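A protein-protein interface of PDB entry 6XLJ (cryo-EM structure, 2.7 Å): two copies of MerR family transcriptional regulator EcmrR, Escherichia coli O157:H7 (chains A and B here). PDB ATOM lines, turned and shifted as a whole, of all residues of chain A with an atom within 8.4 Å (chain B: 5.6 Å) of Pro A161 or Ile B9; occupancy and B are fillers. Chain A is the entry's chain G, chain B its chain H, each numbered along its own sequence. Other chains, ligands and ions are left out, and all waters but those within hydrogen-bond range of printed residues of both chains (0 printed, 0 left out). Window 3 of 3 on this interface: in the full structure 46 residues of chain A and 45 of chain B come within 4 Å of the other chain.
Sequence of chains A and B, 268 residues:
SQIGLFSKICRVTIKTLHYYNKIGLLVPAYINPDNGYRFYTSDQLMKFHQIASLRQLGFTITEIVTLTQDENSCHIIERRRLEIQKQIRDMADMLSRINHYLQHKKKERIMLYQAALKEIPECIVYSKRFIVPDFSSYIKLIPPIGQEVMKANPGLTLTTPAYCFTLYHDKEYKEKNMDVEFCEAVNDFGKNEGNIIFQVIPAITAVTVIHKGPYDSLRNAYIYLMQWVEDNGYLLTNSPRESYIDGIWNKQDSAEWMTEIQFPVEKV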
ATOM      1  N   LYS A 118      35.119  18.819  15.600  1.00  0.00           N
ATOM      2  CA  LYS A 118      34.129  19.348  14.674  1.00  0.00           C
ATOM      3  C   LYS A 118      34.705  20.520  13.886  1.00  0.00           C
ATOM      4  O   LYS A 118      35.680  21.149  14.294  1.00  0.00           O
ATOM      5  CB  LYS A 118      32.856  19.752  15.411  1.00  0.00           C
ATOM      6  CG  LYS A 118      33.035  20.792  16.482  1.00  0.00           C
ATOM      7  CD  LYS A 118      31.726  20.983  17.219  1.00  0.00           C
ATOM      8  CE  LYS A 118      31.191  19.625  17.684  1.00  0.00           C
ATOM      9  NZ  LYS A 118      30.183  19.723  18.772  1.00  0.00           N
ATOM     10  N   GLU A 119      34.093  20.812  12.744  1.00  0.00           N
ATOM     11  CA  GLU A 119      34.529  21.907  11.886  1.00  0.00           C
ATOM     12  C   GLU A 119      33.631  23.116  12.136  1.00  0.00           C
ATOM     13  O   GLU A 119      32.403  22.993  12.169  1.00  0.00           O
ATOM     14  CB  GLU A 119      34.553  21.496  10.409  1.00  0.00           C
ATOM     15  CG  GLU A 119      33.231  21.124   9.769  1.00  0.00           C
ATOM     16  CD  GLU A 119      32.526  22.326   9.179  1.00  0.00           C
ATOM     17  OE1 GLU A 119      33.210  23.341   8.923  1.00  0.00           O
ATOM     18  OE2 GLU A 119      31.296  22.261   8.975  1.00  0.00           O
ATOM     19  N   ILE A 120      34.252  24.261  12.378  1.00  0.00           N
ATOM     20  CA  ILE A 120      33.580  25.537  12.612  1.00  0.00           C
ATOM     21  C   ILE A 120      33.800  26.439  11.402  1.00  0.00           C
ATOM     22  O   ILE A 120      34.950  26.677  11.022  1.00  0.00           O
ATOM     23  CB  ILE A 120      34.110  26.209  13.890  1.00  0.00           C
ATOM     24  CG1 ILE A 120      33.871  25.288  15.085  1.00  0.00           C
ATOM     25  CG2 ILE A 120      33.448  27.557  14.101  1.00  0.00           C
ATOM     26  CD1 ILE A 120      34.731  25.601  16.267  1.00  0.00           C
ATOM     27  N   PRO A 121      32.743  26.960  10.790  1.00  0.00           N
ATOM     28  CA  PRO A 121      32.876  27.816   9.608  1.00  0.00           C
ATOM     29  C   PRO A 121      33.356  29.222   9.955  1.00  0.00           C
ATOM     30  O   PRO A 121      33.401  29.633  11.115  1.00  0.00           O
ATOM     31  CB  PRO A 121      31.454  27.855   9.029  1.00  0.00           C
ATOM     32  CG  PRO A 121      30.660  26.852   9.811  1.00  0.00           C
ATOM     33  CD  PRO A 121      31.333  26.730  11.129  1.00  0.00           C
ATOM     34  N   CYS A 123      33.356  33.333  10.131  1.00  0.00           N
ATOM     35  CA  CYS A 123      32.368  34.258  10.680  1.00  0.00           C
ATOM     36  C   CYS A 123      32.797  35.708  10.456  1.00  0.00           C
ATOM     37  O   CYS A 123      33.960  36.004  10.156  1.00  0.00           O
ATOM     38  CB  CYS A 123      32.140  34.024  12.184  1.00  0.00           C
ATOM     39  SG  CYS A 123      32.076  32.302  12.725  1.00  0.00           S
ATOM     40  N   LEU A 158      23.010  40.322  14.969  1.00  0.00           N
ATOM     41  CA  LEU A 158      23.924  39.228  15.253  1.00  0.00           C
ATOM     42  C   LEU A 158      23.460  37.949  14.564  1.00  0.00           C
ATOM     43  O   LEU A 158      22.268  37.745  14.314  1.00  0.00           O
ATOM     44  CB  LEU A 158      24.099  39.016  16.759  1.00  0.00           C
ATOM     45  CG  LEU A 158      23.068  38.415  17.712  1.00  0.00           C
ATOM     46  CD1 LEU A 158      23.714  38.317  19.079  1.00  0.00           C
ATOM     47  CD2 LEU A 158      21.807  39.256  17.812  1.00  0.00           C
ATOM     48  N   THR A 159      24.422  37.089  14.255  1.00  0.00           N
ATOM     49  CA  THR A 159      24.128  35.831  13.587  1.00  0.00           C
ATOM     50  C   THR A 159      23.327  34.910  14.491  1.00  0.00           C
ATOM     51  O   THR A 159      23.490  34.891  15.712  1.00  0.00           O
ATOM     52  CB  THR A 159      25.419  35.128  13.167  1.00  0.00           C
ATOM     53  OG1 THR A 159      26.276  34.970  14.306  1.00  0.00           O
ATOM     54  CG2 THR A 159      26.136  35.913  12.095  1.00  0.00           C
ATOM     55  N   THR A 160      22.441  34.145  13.861  1.00  0.00           N
ATOM     56  CA  THR A 160      21.626  33.150  14.534  1.00  0.00           C
ATOM     57  C   THR A 160      21.934  31.809  13.892  1.00  0.00           C
ATOM     58  O   THR A 160      21.652  31.618  12.697  1.00  0.00           O
ATOM     59  CB  THR A 160      20.132  33.465  14.405  1.00  0.00           C
ATOM     60  OG1 THR A 160      19.689  33.152  13.078  1.00  0.00           O
ATOM     61  CG2 THR A 160      19.854  34.934  14.694  1.00  0.00           C
ATOM     62  N   PRO A 161      22.506  30.852  14.633  1.00  0.00           N
ATOM     63  CA  PRO A 161      22.758  30.866  16.082  1.00  0.00           C
ATOM     64  C   PRO A 161      23.890  31.790  16.565  1.00  0.00           C
ATOM     65  O   PRO A 161      24.828  32.074  15.822  1.00  0.00           O
ATOM     66  CB  PRO A 161      23.121  29.410  16.366  1.00  0.00           C
ATOM     67  CG  PRO A 161      23.785  28.966  15.118  1.00  0.00           C
ATOM     68  CD  PRO A 161      23.067  29.652  13.993  1.00  0.00           C
ATOM     69  N   ALA A 162      23.767  32.271  17.800  1.00  0.00           N
ATOM     70  CA  ALA A 162      24.694  33.260  18.331  1.00  0.00           C
ATOM     71  C   ALA A 162      26.045  32.606  18.586  1.00  0.00           C
ATOM     72  O   ALA A 162      26.122  31.553  19.226  1.00  0.00           O
ATOM     73  CB  ALA A 162      24.143  33.876  19.613  1.00  0.00           C
ATOM     74  N   TYR A 163      27.110  33.213  18.072  1.00  0.00           N
ATOM     75  CA  TYR A 163      28.463  32.725  18.327  1.00  0.00           C
ATOM     76  C   TYR A 163      29.230  33.811  19.080  1.00  0.00           C
ATOM     77  O   TYR A 163      29.647  34.811  18.487  1.00  0.00           O
ATOM     78  CB  TYR A 163      29.146  32.374  17.008  1.00  0.00           C
ATOM     79  CG  TYR A 163      30.400  31.547  17.131  1.00  0.00           C
ATOM     80  CD1 TYR A 163      30.712  30.895  18.312  1.00  0.00           C
ATOM     81  CD2 TYR A 163      31.255  31.392  16.052  1.00  0.00           C
ATOM     82  CE1 TYR A 163      31.843  30.123  18.417  1.00  0.00           C
ATOM     83  CE2 TYR A 163      32.393  30.623  16.150  1.00  0.00           C
ATOM     84  CZ  TYR A 163      32.684  29.992  17.336  1.00  0.00           C
ATOM     85  OH  TYR A 163      33.818  29.219  17.441  1.00  0.00           O
ATOM     86  N   CYS A 164      29.392  33.627  20.391  1.00  0.00           N
ATOM     87  CA  CYS A 164      30.042  34.605  21.262  1.00  0.00           C
ATOM     88  C   CYS A 164      31.149  33.907  22.045  1.00  0.00           C
ATOM     89  O   CYS A 164      30.874  33.098  22.941  1.00  0.00           O
ATOM     90  CB  CYS A 164      29.023  35.273  22.185  1.00  0.00           C
ATOM     91  SG  CYS A 164      28.030  34.142  23.185  1.00  0.00           S
ATOM     92  N   GLU A 184      32.486  38.371  18.832  1.00  0.00           N
ATOM     93  CA  GLU A 184      31.105  37.937  18.662  1.00  0.00           C
ATOM     94  C   GLU A 184      30.689  38.128  17.215  1.00  0.00           C
ATOM     95  O   GLU A 184      30.913  39.198  16.646  1.00  0.00           O
ATOM     96  CB  GLU A 184      30.153  38.686  19.598  1.00  0.00           C
ATOM     97  CG  GLU A 184      28.713  38.197  19.520  1.00  0.00           C
ATOM     98  CD  GLU A 184      27.824  38.843  20.562  1.00  0.00           C
ATOM     99  OE1 GLU A 184      28.305  39.757  21.260  1.00  0.00           O
ATOM    100  OE2 GLU A 184      26.652  38.430  20.686  1.00  0.00           O
ATOM    101  N   ALA A 185      30.054  37.111  16.638  1.00  0.00           N
ATOM    102  CA  ALA A 185      29.775  37.094  15.208  1.00  0.00           C
ATOM    103  C   ALA A 185      28.501  37.858  14.883  1.00  0.00           C
ATOM    104  O   ALA A 185      27.472  37.674  15.537  1.00  0.00           O
ATOM    105  CB  ALA A 185      29.652  35.657  14.711  1.00  0.00           C
ATOM    106  N   VAL A 186      28.569  38.702  13.853  1.00  0.00           N
ATOM    107  CA  VAL A 186      27.420  39.420  13.323  1.00  0.00           C
ATOM    108  C   VAL A 186      27.316  39.165  11.822  1.00  0.00           C
ATOM    109  O   VAL A 186      28.134  38.464  11.230  1.00  0.00           O
ATOM    110  CB  VAL A 186      27.480  40.929  13.621  1.00  0.00           C
ATOM    111  CG1 VAL A 186      27.383  41.170  15.108  1.00  0.00           C
ATOM    112  CG2 VAL A 186      28.763  41.517  13.073  1.00  0.00           C
ATOM    113  N   ASN A 187      26.291  39.759  11.213  1.00  0.00           N
ATOM    114  CA  ASN A 187      25.942  39.518   9.819  1.00  0.00           C
ATOM    115  C   ASN A 187      26.704  40.410   8.845  1.00  0.00           C
ATOM    116  O   ASN A 187      27.233  39.927   7.840  1.00  0.00           O
ATOM    117  CB  ASN A 187      24.438  39.738   9.611  1.00  0.00           C
ATOM    118  CG  ASN A 187      23.589  38.715  10.327  1.00  0.00           C
ATOM    119  OD1 ASN A 187      23.988  38.169  11.350  1.00  0.00           O
ATOM    120  ND2 ASN A 187      22.398  38.461   9.799  1.00  0.00           N
ATOM    121  N   ILE A 245      27.415  28.906  25.380  1.00  0.00           N
ATOM    122  CA  ILE A 245      26.085  28.387  25.096  1.00  0.00           C
ATOM    123  C   ILE A 245      25.101  28.941  26.109  1.00  0.00           C
ATOM    124  O   ILE A 245      24.148  29.650  25.763  1.00  0.00           O
ATOM    125  CB  ILE A 245      26.080  26.850  25.122  1.00  0.00           C
ATOM    126  CG1 ILE A 245      27.272  26.278  24.367  1.00  0.00           C
ATOM    127  CG2 ILE A 245      24.783  26.319  24.561  1.00  0.00           C
ATOM    128  CD1 ILE A 245      27.452  24.799  24.595  1.00  0.00           C
ATOM    129  N   GLU A 260      31.619  25.963  25.793  1.00  0.00           N
ATOM    130  CA  GLU A 260      32.297  24.968  24.972  1.00  0.00           C
ATOM    131  C   GLU A 260      33.667  25.484  24.553  1.00  0.00           C
ATOM    132  O   GLU A 260      33.780  26.485  23.839  1.00  0.00           O
ATOM    133  CB  GLU A 260      31.409  24.547  23.800  1.00  0.00           C
ATOM    134  CG  GLU A 260      31.044  25.544  22.744  1.00  0.00           C
ATOM    135  CD  GLU A 260      31.842  25.303  21.500  1.00  0.00           C
ATOM    136  OE1 GLU A 260      32.641  24.351  21.504  1.00  0.00           O
ATOM    137  OE2 GLU A 260      31.646  26.018  20.501  1.00  0.00           O
ATOM    138  N   SER B   1      13.681  27.092  20.298  1.00  0.00           N
ATOM    139  CA  SER B   1      14.589  26.509  19.319  1.00  0.00           C
ATOM    140  C   SER B   1      13.946  25.312  18.643  1.00  0.00           C
ATOM    141  O   SER B   1      13.997  24.194  19.157  1.00  0.00           O
ATOM    142  CB  SER B   1      15.903  26.087  19.973  1.00  0.00           C
ATOM    143  OG  SER B   1      15.813  24.763  20.458  1.00  0.00           O
ATOM    144  N   GLY B   4      15.077  23.394  13.189  1.00  0.00           N
ATOM    145  CA  GLY B   4      15.964  24.027  12.228  1.00  0.00           C
ATOM    146  C   GLY B   4      17.091  24.791  12.896  1.00  0.00           C
ATOM    147  O   GLY B   4      18.257  24.659  12.515  1.00  0.00           O
ATOM    148  N   LEU B   5      16.766  25.579  13.914  1.00  0.00           N
ATOM    149  CA  LEU B   5      17.800  26.322  14.623  1.00  0.00           C
ATOM    150  C   LEU B   5      18.722  25.379  15.385  1.00  0.00           C
ATOM    151  O   LEU B   5      19.933  25.613  15.466  1.00  0.00           O
ATOM    152  CB  LEU B   5      17.160  27.363  15.533  1.00  0.00           C
ATOM    153  CG  LEU B   5      16.528  28.436  14.639  1.00  0.00           C
ATOM    154  CD1 LEU B   5      15.692  29.424  15.427  1.00  0.00           C
ATOM    155  CD2 LEU B   5      17.607  29.158  13.843  1.00  0.00           C
ATOM    156  N   PHE B   6      18.168  24.297  15.931  1.00  0.00           N
ATOM    157  CA  PHE B   6      18.999  23.311  16.609  1.00  0.00           C
ATOM    158  C   PHE B   6      19.900  22.589  15.618  1.00  0.00           C
ATOM    159  O   PHE B   6      21.072  22.331  15.911  1.00  0.00           O
ATOM    160  CB  PHE B   6      18.110  22.328  17.352  1.00  0.00           C
ATOM    161  CG  PHE B   6      18.817  21.554  18.403  1.00  0.00           C
ATOM    162  CD1 PHE B   6      19.315  22.179  19.524  1.00  0.00           C
ATOM    163  CD2 PHE B   6      18.956  20.193  18.289  1.00  0.00           C
ATOM    164  CE1 PHE B   6      19.958  21.456  20.502  1.00  0.00           C
ATOM    165  CE2 PHE B   6      19.592  19.465  19.257  1.00  0.00           C
ATOM    166  CZ  PHE B   6      20.095  20.094  20.366  1.00  0.00           C
ATOM    167  N   SER B   7      19.368  22.257  14.440  1.00  0.00           N
ATOM    168  CA  SER B   7      20.155  21.596  13.407  1.00  0.00           C
ATOM    169  C   SER B   7      21.237  22.515  12.878  1.00  0.00           C
ATOM    170  O   SER B   7      22.259  22.048  12.367  1.00  0.00           O
ATOM    171  CB  SER B   7      19.256  21.160  12.258  1.00  0.00           C
ATOM    172  OG  SER B   7      18.585  22.275  11.711  1.00  0.00           O
ATOM    173  N   LYS B   8      21.023  23.821  12.979  1.00  0.00           N
ATOM    174  CA  LYS B   8      22.051  24.781  12.618  1.00  0.00           C
ATOM    175  C   LYS B   8      23.048  25.019  13.737  1.00  0.00           C
ATOM    176  O   LYS B   8      24.158  25.482  13.459  1.00  0.00           O
ATOM    177  CB  LYS B   8      21.423  26.103  12.189  1.00  0.00           C
ATOM    178  CG  LYS B   8      20.738  26.025  10.843  1.00  0.00           C
ATOM    179  CD  LYS B   8      20.227  27.372  10.392  1.00  0.00           C
ATOM    180  CE  LYS B   8      19.648  27.278   9.002  1.00  0.00           C
ATOM    181  NZ  LYS B   8      19.175  28.601   8.522  1.00  0.00           N
ATOM    182  N   ILE B   9      22.681  24.735  14.986  1.00  0.00           N
ATOM    183  CA  ILE B   9      23.654  24.839  16.069  1.00  0.00           C
ATOM    184  C   ILE B   9      24.696  23.743  15.929  1.00  0.00           C
ATOM    185  O   ILE B   9      25.903  24.006  15.917  1.00  0.00           O
ATOM    186  CB  ILE B   9      22.945  24.754  17.433  1.00  0.00           C
ATOM    187  CG1 ILE B   9      22.244  26.065  17.766  1.00  0.00           C
ATOM    188  CG2 ILE B   9      23.918  24.392  18.534  1.00  0.00           C
ATOM    189  CD1 ILE B   9      21.375  25.979  19.001  1.00  0.00           C
ATOM    190  N   CYS B  10      24.243  22.497  15.821  1.00  0.00           N
ATOM    191  CA  CYS B  10      25.130  21.349  15.717  1.00  0.00           C
ATOM    192  C   CYS B  10      25.743  21.186  14.330  1.00  0.00           C
ATOM    193  O   CYS B  10      26.609  20.320  14.170  1.00  0.00           O
ATOM    194  CB  CYS B  10      24.393  20.084  16.139  1.00  0.00           C
ATOM    195  SG  CYS B  10      23.349  20.287  17.586  1.00  0.00           S
ATOM    196  N   ARG B  11      25.315  21.983  13.342  1.00  0.00           N
ATOM    197  CA  ARG B  11      25.696  21.822  11.932  1.00  0.00           C
ATOM    198  C   ARG B  11      25.381  20.416  11.439  1.00  0.00           C
ATOM    199  O   ARG B  11      26.196  19.754  10.794  1.00  0.00           O
ATOM    200  CB  ARG B  11      27.170  22.158  11.727  1.00  0.00           C
ATOM    201  CG  ARG B  11      27.514  23.558  12.151  1.00  0.00           C
ATOM    202  CD  ARG B  11      29.003  23.741  12.246  1.00  0.00           C
ATOM    203  NE  ARG B  11      29.354  24.968  12.954  1.00  0.00           N
ATOM    204  CZ  ARG B  11      29.457  25.077  14.275  1.00  0.00           C
ATOM    205  NH1 ARG B  11      29.238  24.028  15.060  1.00  0.00           N
ATOM    206  NH2 ARG B  11      29.794  26.242  14.810  1.00  0.00           N
ATOM    207  N   LEU B  45      21.480  19.470  23.546  1.00  0.00           N
ATOM    208  CA  LEU B  45      22.754  19.702  22.879  1.00  0.00           C
ATOM    209  C   LEU B  45      23.866  18.972  23.618  1.00  0.00           C
ATOM    210  O   LEU B  45      24.762  18.398  22.995  1.00  0.00           O
ATOM    211  CB  LEU B  45      23.058  21.193  22.785  1.00  0.00           C
ATOM    212  CG  LEU B  45      24.512  21.573  22.499  1.00  0.00           C
ATOM    213  CD1 LEU B  45      24.963  21.061  21.138  1.00  0.00           C
ATOM    214  CD2 LEU B  45      24.689  23.066  22.598  1.00  0.00           C
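O of Pro A121 is in hydrogen-bond range of SG of Cys A123 (3.4 Å). The guanidinium group (NH1) of Arg B11 is in hydrogen-bond range of the backbone carbonyl oxygen (O) of Ile B9, 3.4 Å away.
Arg B11 touches Glu A119 (CD to O, 3.5 Å). Ile A120 touches Arg B11. NE of Arg B11 touches CD of Pro A121, at 3.2 Å. Lys B8 touches Pro A161. CB of Pro A161 touches CG1 of Ile B9, at 3.7 Å. CD2 of Leu B45 touches CG2 of Ile A245 (3.8 Å).
Printed residues of chain B within 4 Å of Glu A119: Arg B11. Of the printed residues of chain B, Pro A121 touches Arg B11 (3.2 Å). Of chain B, only Lys B8 and Ile B9 come within 4 Å of Pro A161. Glu A184 touches none of the printed residues of chain B. Ala A185 touches none of the printed residues of chain B. Ile B9 touches one residue of chain A. No residue of chain A comes within 4 Å of Cys B10. Of the printed residues of chain A, Leu B45 touches Ile A245 (3.8 Å). The nearest residue of chain B that does not touch Pro A161 is Leu B5 (5.0 Å). The nearest printed residue of chain A that does not touch Ile B9 is Ile A245 (6.4 Å).
Of the 18 printed residues of chain A, 5 touch a printed residue of chain B. Hydrophobic or aromatic side chains of chain A that line the printed part of chain B: Ile A120, Pro A121, Pro A161 and Ile A245. Among the printed residues, no Asp or Glu carboxylate lies within 4 Å of a Lys or Arg side-chain nitrogen of the other chain.
No position is printed for both chains. Of the 6 pairs that touch across the chains among the printed residues, none has its exchanged pair printed and touching as well.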
